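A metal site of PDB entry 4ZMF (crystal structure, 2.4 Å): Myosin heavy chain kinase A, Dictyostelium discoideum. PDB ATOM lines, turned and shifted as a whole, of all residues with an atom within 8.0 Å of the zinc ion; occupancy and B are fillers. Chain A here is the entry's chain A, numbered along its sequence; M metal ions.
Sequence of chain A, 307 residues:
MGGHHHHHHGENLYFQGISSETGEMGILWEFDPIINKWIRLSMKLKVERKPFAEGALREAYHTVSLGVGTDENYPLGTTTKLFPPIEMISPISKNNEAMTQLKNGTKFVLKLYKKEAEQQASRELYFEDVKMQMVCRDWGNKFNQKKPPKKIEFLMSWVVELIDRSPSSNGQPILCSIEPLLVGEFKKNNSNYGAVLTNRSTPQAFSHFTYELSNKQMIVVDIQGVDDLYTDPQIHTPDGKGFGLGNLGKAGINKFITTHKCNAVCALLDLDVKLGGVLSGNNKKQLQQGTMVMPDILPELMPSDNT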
ATOM      1  N   SER A 201       7.569 -24.885 -25.230  1.00  0.00           N
ATOM      2  CA  SER A 201       6.640 -25.106 -24.127  1.00  0.00           C
ATOM      3  C   SER A 201       5.649 -26.269 -24.314  1.00  0.00           C
ATOM      4  O   SER A 201       5.365 -27.012 -23.365  1.00  0.00           O
ATOM      5  CB  SER A 201       5.818 -23.825 -23.928  1.00  0.00           C
ATOM      6  OG  SER A 201       6.616 -22.772 -23.416  1.00  0.00           O
ATOM      7  N   GLN A 204       6.349 -29.920 -23.218  1.00  0.00           N
ATOM      8  CA  GLN A 204       6.564 -30.120 -21.796  1.00  0.00           C
ATOM      9  C   GLN A 204       5.260 -29.935 -21.074  1.00  0.00           C
ATOM     10  O   GLN A 204       4.977 -30.615 -20.104  1.00  0.00           O
ATOM     11  CB  GLN A 204       7.620 -29.161 -21.238  1.00  0.00           C
ATOM     12  CG  GLN A 204       8.949 -29.140 -21.987  1.00  0.00           C
ATOM     13  CD  GLN A 204       9.615 -30.484 -22.090  1.00  0.00           C
ATOM     14  OE1 GLN A 204       9.513 -31.349 -21.187  1.00  0.00           O
ATOM     15  NE2 GLN A 204      10.305 -30.699 -23.186  1.00  0.00           N
ATOM     16  N   ALA A 205       4.466 -28.988 -21.533  1.00  0.00           N
ATOM     17  CA  ALA A 205       3.163 -28.773 -20.950  1.00  0.00           C
ATOM     18  C   ALA A 205       2.235 -29.978 -21.219  1.00  0.00           C
ATOM     19  O   ALA A 205       1.429 -30.355 -20.372  1.00  0.00           O
ATOM     20  CB  ALA A 205       2.547 -27.481 -21.476  1.00  0.00           C
ATOM     21  N   PHE A 206       2.369 -30.591 -22.381  1.00  0.00           N
ATOM     22  CA  PHE A 206       1.592 -31.790 -22.670  1.00  0.00           C
ATOM     23  C   PHE A 206       1.965 -32.901 -21.713  1.00  0.00           C
ATOM     24  O   PHE A 206       1.101 -33.535 -21.145  1.00  0.00           O
ATOM     25  CB  PHE A 206       1.774 -32.261 -24.121  1.00  0.00           C
ATOM     26  CG  PHE A 206       1.133 -33.587 -24.387  1.00  0.00           C
ATOM     27  CD1 PHE A 206      -0.244 -33.700 -24.441  1.00  0.00           C
ATOM     28  CD2 PHE A 206       1.894 -34.730 -24.534  1.00  0.00           C
ATOM     29  CE1 PHE A 206      -0.855 -34.924 -24.644  1.00  0.00           C
ATOM     30  CE2 PHE A 206       1.314 -35.965 -24.740  1.00  0.00           C
ATOM     31  CZ  PHE A 206      -0.076 -36.061 -24.780  1.00  0.00           C
ATOM     32  N   SER A 207       3.248 -33.152 -21.511  1.00  0.00           N
ATOM     33  CA  SER A 207       3.642 -34.180 -20.564  1.00  0.00           C
ATOM     34  C   SER A 207       3.082 -33.897 -19.178  1.00  0.00           C
ATOM     35  O   SER A 207       2.529 -34.804 -18.532  1.00  0.00           O
ATOM     36  CB  SER A 207       5.146 -34.321 -20.505  1.00  0.00           C
ATOM     37  OG  SER A 207       5.636 -34.707 -21.768  1.00  0.00           O
ATOM     38  N   HIS A 208       3.177 -32.657 -18.744  1.00  0.00           N
ATOM     39  CA  HIS A 208       2.662 -32.304 -17.427  1.00  0.00           C
ATOM     40  C   HIS A 208       1.140 -32.500 -17.357  1.00  0.00           C
ATOM     41  O   HIS A 208       0.644 -33.132 -16.440  1.00  0.00           O
ATOM     42  CB  HIS A 208       3.093 -30.884 -17.049  1.00  0.00           C
ATOM     43  CG  HIS A 208       2.689 -30.481 -15.671  1.00  0.00           C
ATOM     44  ND1 HIS A 208       2.766 -29.183 -15.226  1.00  0.00           N
ATOM     45  CD2 HIS A 208       2.199 -31.207 -14.642  1.00  0.00           C
ATOM     46  CE1 HIS A 208       2.317 -29.119 -13.987  1.00  0.00           C
ATOM     47  NE2 HIS A 208       1.967 -30.335 -13.606  1.00  0.00           N
ATOM     48  N   PHE A 209       0.424 -32.017 -18.374  1.00  0.00           N
ATOM     49  CA  PHE A 209      -1.032 -32.262 -18.509  1.00  0.00           C
ATOM     50  C   PHE A 209      -1.393 -33.741 -18.295  1.00  0.00           C
ATOM     51  O   PHE A 209      -2.274 -34.057 -17.504  1.00  0.00           O
ATOM     52  CB  PHE A 209      -1.472 -31.835 -19.917  1.00  0.00           C
ATOM     53  CG  PHE A 209      -2.954 -31.981 -20.204  1.00  0.00           C
ATOM     54  CD1 PHE A 209      -3.849 -31.014 -19.790  1.00  0.00           C
ATOM     55  CD2 PHE A 209      -3.416 -33.023 -20.973  1.00  0.00           C
ATOM     56  CE1 PHE A 209      -5.193 -31.119 -20.090  1.00  0.00           C
ATOM     57  CE2 PHE A 209      -4.746 -33.144 -21.262  1.00  0.00           C
ATOM     58  CZ  PHE A 209      -5.635 -32.192 -20.833  1.00  0.00           C
ATOM     59  N   GLU A 212      -1.072 -34.745 -14.592  1.00  0.00           N
ATOM     60  CA  GLU A 212      -2.065 -34.206 -13.688  1.00  0.00           C
ATOM     61  C   GLU A 212      -3.473 -34.740 -13.977  1.00  0.00           C
ATOM     62  O   GLU A 212      -4.164 -35.210 -13.074  1.00  0.00           O
ATOM     63  CB  GLU A 212      -2.069 -32.669 -13.656  1.00  0.00           C
ATOM     64  CG  GLU A 212      -3.003 -32.122 -12.578  1.00  0.00           C
ATOM     65  CD  GLU A 212      -2.926 -30.614 -12.360  1.00  0.00           C
ATOM     66  OE1 GLU A 212      -3.998 -29.957 -12.217  1.00  0.00           O
ATOM     67  OE2 GLU A 212      -1.798 -30.074 -12.301  1.00  0.00           O
ATOM     68  N   PHE A 256      10.891 -37.096 -14.461  1.00  0.00           N
ATOM     69  CA  PHE A 256      10.212 -36.033 -15.200  1.00  0.00           C
ATOM     70  C   PHE A 256       9.958 -34.820 -14.307  1.00  0.00           C
ATOM     71  O   PHE A 256      10.159 -33.661 -14.711  1.00  0.00           O
ATOM     72  CB  PHE A 256       8.874 -36.470 -15.785  1.00  0.00           C
ATOM     73  CG  PHE A 256       8.135 -35.343 -16.441  1.00  0.00           C
ATOM     74  CD1 PHE A 256       8.449 -34.954 -17.729  1.00  0.00           C
ATOM     75  CD2 PHE A 256       7.222 -34.597 -15.722  1.00  0.00           C
ATOM     76  CE1 PHE A 256       7.827 -33.856 -18.306  1.00  0.00           C
ATOM     77  CE2 PHE A 256       6.600 -33.508 -16.295  1.00  0.00           C
ATOM     78  CZ  PHE A 256       6.896 -33.134 -17.591  1.00  0.00           C
ATOM     79  N   HIS A 260      11.203 -30.606 -14.579  1.00  0.00           N
ATOM     80  CA  HIS A 260      10.123 -29.881 -15.218  1.00  0.00           C
ATOM     81  C   HIS A 260       9.992 -28.499 -14.609  1.00  0.00           C
ATOM     82  O   HIS A 260       9.904 -28.374 -13.402  1.00  0.00           O
ATOM     83  CB  HIS A 260       8.790 -30.639 -15.110  1.00  0.00           C
ATOM     84  CG  HIS A 260       7.646 -29.880 -15.687  1.00  0.00           C
ATOM     85  ND1 HIS A 260       7.500 -29.653 -17.051  1.00  0.00           N
ATOM     86  CD2 HIS A 260       6.597 -29.254 -15.096  1.00  0.00           C
ATOM     87  CE1 HIS A 260       6.407 -28.934 -17.257  1.00  0.00           C
ATOM     88  NE2 HIS A 260       5.841 -28.687 -16.088  1.00  0.00           N
ATOM     89  N   LYS A 261       9.970 -27.482 -15.476  1.00  0.00           N
ATOM     90  CA  LYS A 261       9.642 -26.106 -15.131  1.00  0.00           C
ATOM     91  C   LYS A 261       8.362 -25.749 -15.890  1.00  0.00           C
ATOM     92  O   LYS A 261       8.328 -25.835 -17.126  1.00  0.00           O
ATOM     93  CB  LYS A 261      10.752 -25.141 -15.566  1.00  0.00           C
ATOM     94  CG  LYS A 261      12.130 -25.329 -14.900  1.00  0.00           C
ATOM     95  CD  LYS A 261      13.045 -24.091 -14.973  1.00  0.00           C
ATOM     96  CE  LYS A 261      13.049 -23.393 -16.330  1.00  0.00           C
ATOM     97  NZ  LYS A 261      14.034 -22.265 -16.385  1.00  0.00           N
ATOM     98  N   CYS A 262       7.334 -25.327 -15.163  1.00  0.00           N
ATOM     99  CA  CYS A 262       6.070 -24.967 -15.784  1.00  0.00           C
ATOM    100  C   CYS A 262       6.264 -23.724 -16.667  1.00  0.00           C
ATOM    101  O   CYS A 262       7.123 -22.869 -16.406  1.00  0.00           O
ATOM    102  CB  CYS A 262       4.951 -24.770 -14.757  1.00  0.00           C
ATOM    103  SG  CYS A 262       4.262 -26.290 -14.042  1.00  0.00           S
ATOM    104  N   ASN A 263       5.459 -23.633 -17.712  1.00  0.00           N
ATOM    105  CA  ASN A 263       5.602 -22.565 -18.676  1.00  0.00           C
ATOM    106  C   ASN A 263       4.239 -21.956 -18.896  1.00  0.00           C
ATOM    107  O   ASN A 263       3.285 -22.323 -18.226  1.00  0.00           O
ATOM    108  CB  ASN A 263       6.217 -23.121 -19.967  1.00  0.00           C
ATOM    109  CG  ASN A 263       5.402 -24.273 -20.563  1.00  0.00           C
ATOM    110  OD1 ASN A 263       4.188 -24.142 -20.744  1.00  0.00           O
ATOM    111  ND2 ASN A 263       6.058 -25.383 -20.835  1.00  0.00           N
ATOM    112  N   ALA A 264       4.138 -21.045 -19.832  1.00  0.00           N
ATOM    113  CA  ALA A 264       2.890 -20.350 -20.059  1.00  0.00           C
ATOM    114  C   ALA A 264       1.735 -21.275 -20.447  1.00  0.00           C
ATOM    115  O   ALA A 264       0.578 -21.052 -20.092  1.00  0.00           O
ATOM    116  CB  ALA A 264       3.113 -19.291 -21.129  1.00  0.00           C
ATOM    117  N   VAL A 265       2.056 -22.364 -21.147  1.00  0.00           N
ATOM    118  CA  VAL A 265       1.023 -23.327 -21.530  1.00  0.00           C
ATOM    119  C   VAL A 265       0.520 -24.069 -20.301  1.00  0.00           C
ATOM    120  O   VAL A 265      -0.680 -24.235 -20.127  1.00  0.00           O
ATOM    121  CB  VAL A 265       1.511 -24.286 -22.635  1.00  0.00           C
ATOM    122  CG1 VAL A 265       0.419 -25.278 -23.007  1.00  0.00           C
ATOM    123  CG2 VAL A 265       1.914 -23.496 -23.874  1.00  0.00           C
ATOM    124  N   CYS A 266       1.417 -24.494 -19.418  1.00  0.00           N
ATOM    125  CA  CYS A 266       0.986 -25.132 -18.177  1.00  0.00           C
ATOM    126  C   CYS A 266       0.009 -24.228 -17.438  1.00  0.00           C
ATOM    127  O   CYS A 266      -1.010 -24.693 -16.923  1.00  0.00           O
ATOM    128  CB  CYS A 266       2.164 -25.468 -17.228  1.00  0.00           C
ATOM    129  SG  CYS A 266       3.442 -26.562 -17.869  1.00  0.00           S
ATOM    130  N   ALA A 267       0.347 -22.947 -17.341  1.00  0.00           N
ATOM    131  CA  ALA A 267      -0.464 -21.971 -16.596  1.00  0.00           C
ATOM    132  C   ALA A 267      -1.815 -21.771 -17.258  1.00  0.00           C
ATOM    133  O   ALA A 267      -2.844 -21.721 -16.596  1.00  0.00           O
ATOM    134  CB  ALA A 267       0.258 -20.621 -16.488  1.00  0.00           C
ATOM    135  N   LEU A 269      -3.377 -23.928 -18.965  1.00  0.00           N
ATOM    136  CA  LEU A 269      -4.152 -25.148 -18.673  1.00  0.00           C
ATOM    137  C   LEU A 269      -4.435 -25.324 -17.184  1.00  0.00           C
ATOM    138  O   LEU A 269      -4.909 -26.370 -16.751  1.00  0.00           O
ATOM    139  CB  LEU A 269      -3.391 -26.375 -19.183  1.00  0.00           C
ATOM    140  CG  LEU A 269      -3.125 -26.396 -20.677  1.00  0.00           C
ATOM    141  CD1 LEU A 269      -2.128 -27.467 -21.034  1.00  0.00           C
ATOM    142  CD2 LEU A 269      -4.409 -26.622 -21.409  1.00  0.00           C
ATOM    143  N   LEU A 271      -2.563 -25.827 -14.631  1.00  0.00           N
ATOM    144  CA  LEU A 271      -1.892 -26.955 -13.971  1.00  0.00           C
ATOM    145  C   LEU A 271      -1.187 -26.493 -12.704  1.00  0.00           C
ATOM    146  O   LEU A 271      -0.736 -25.340 -12.585  1.00  0.00           O
ATOM    147  CB  LEU A 271      -0.887 -27.628 -14.913  1.00  0.00           C
ATOM    148  CG  LEU A 271      -1.439 -28.257 -16.202  1.00  0.00           C
ATOM    149  CD1 LEU A 271      -0.328 -28.830 -17.064  1.00  0.00           C
ATOM    150  CD2 LEU A 271      -2.484 -29.333 -15.909  1.00  0.00           C
ATOM    151  N   ASP A 272      -1.086 -27.430 -11.781  1.00  0.00           N
ATOM    152  CA  ASP A 272      -0.529 -27.222 -10.465  1.00  0.00           C
ATOM    153  C   ASP A 272       0.982 -27.124 -10.587  1.00  0.00           C
ATOM    154  O   ASP A 272       1.601 -28.015 -11.140  1.00  0.00           O
ATOM    155  CB  ASP A 272      -0.916 -28.413  -9.575  1.00  0.00           C
ATOM    156  CG  ASP A 272      -0.912 -28.084  -8.113  1.00  0.00           C
ATOM    157  OD1 ASP A 272       0.051 -27.405  -7.654  1.00  0.00           O
ATOM    158  OD2 ASP A 272      -1.860 -28.503  -7.412  1.00  0.00           O
ATOM    159  N   VAL A 273       1.580 -26.073 -10.040  1.00  0.00           N
ATOM    160  CA  VAL A 273       3.039 -25.900 -10.137  1.00  0.00           C
ATOM    161  C   VAL A 273       3.826 -26.927  -9.292  1.00  0.00           C
ATOM    162  O   VAL A 273       5.047 -27.049  -9.430  1.00  0.00           O
ATOM    163  CB  VAL A 273       3.453 -24.452  -9.822  1.00  0.00           C
ATOM    164  CG1 VAL A 273       4.952 -24.277  -9.994  1.00  0.00           C
ATOM    165  CG2 VAL A 273       2.734 -23.474 -10.737  1.00  0.00           C
ATOM    166  N   LYS A 274       3.130 -27.701  -8.442  1.00  0.00           N
ATOM    167  CA  LYS A 274       3.710 -28.976  -7.926  1.00  0.00           C
ATOM    168  C   LYS A 274       3.979 -29.944  -9.118  1.00  0.00           C
ATOM    169  O   LYS A 274       3.808 -31.175  -9.025  1.00  0.00           O
ATOM    170  CB  LYS A 274       2.790 -29.636  -6.890  1.00  0.00           C
ATOM    171  CG  LYS A 274       2.916 -29.130  -5.454  1.00  0.00           C
ATOM    172  CD  LYS A 274       2.139 -29.981  -4.447  1.00  0.00           C
ATOM    173  CE  LYS A 274       0.840 -30.610  -4.974  1.00  0.00           C
ATOM    174  NZ  LYS A 274      -0.289 -29.645  -5.052  1.00  0.00           N
HETATM  175 ZN    ZN M   1       4.014 -27.626 -16.046  1.00  0.00          ZN
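The zinc ion is bound by NE2 of His 260 (2.1 Å), ND1 of His 208 (2.2 Å), SG of Cys 266 (2.2 Å) and SG of Cys 262 (2.4 Å).
The backbone NH (N) of Cys 266 sits at hydrogen-bond distance from the side-chain amide oxygen (OD1) of Asn 263 (3.1 Å).
The backbone carbonyl oxygen of Asp 272 lies close to a ring nitrogen (NE2) of His 208, at 3.4 Å.
N of Leu 271 is in hydrogen-bond range of O of Cys 266, at 3.0 Å.
The nearest printed residue that does not touch the zinc ion is Asn 263 (4.6 Å).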
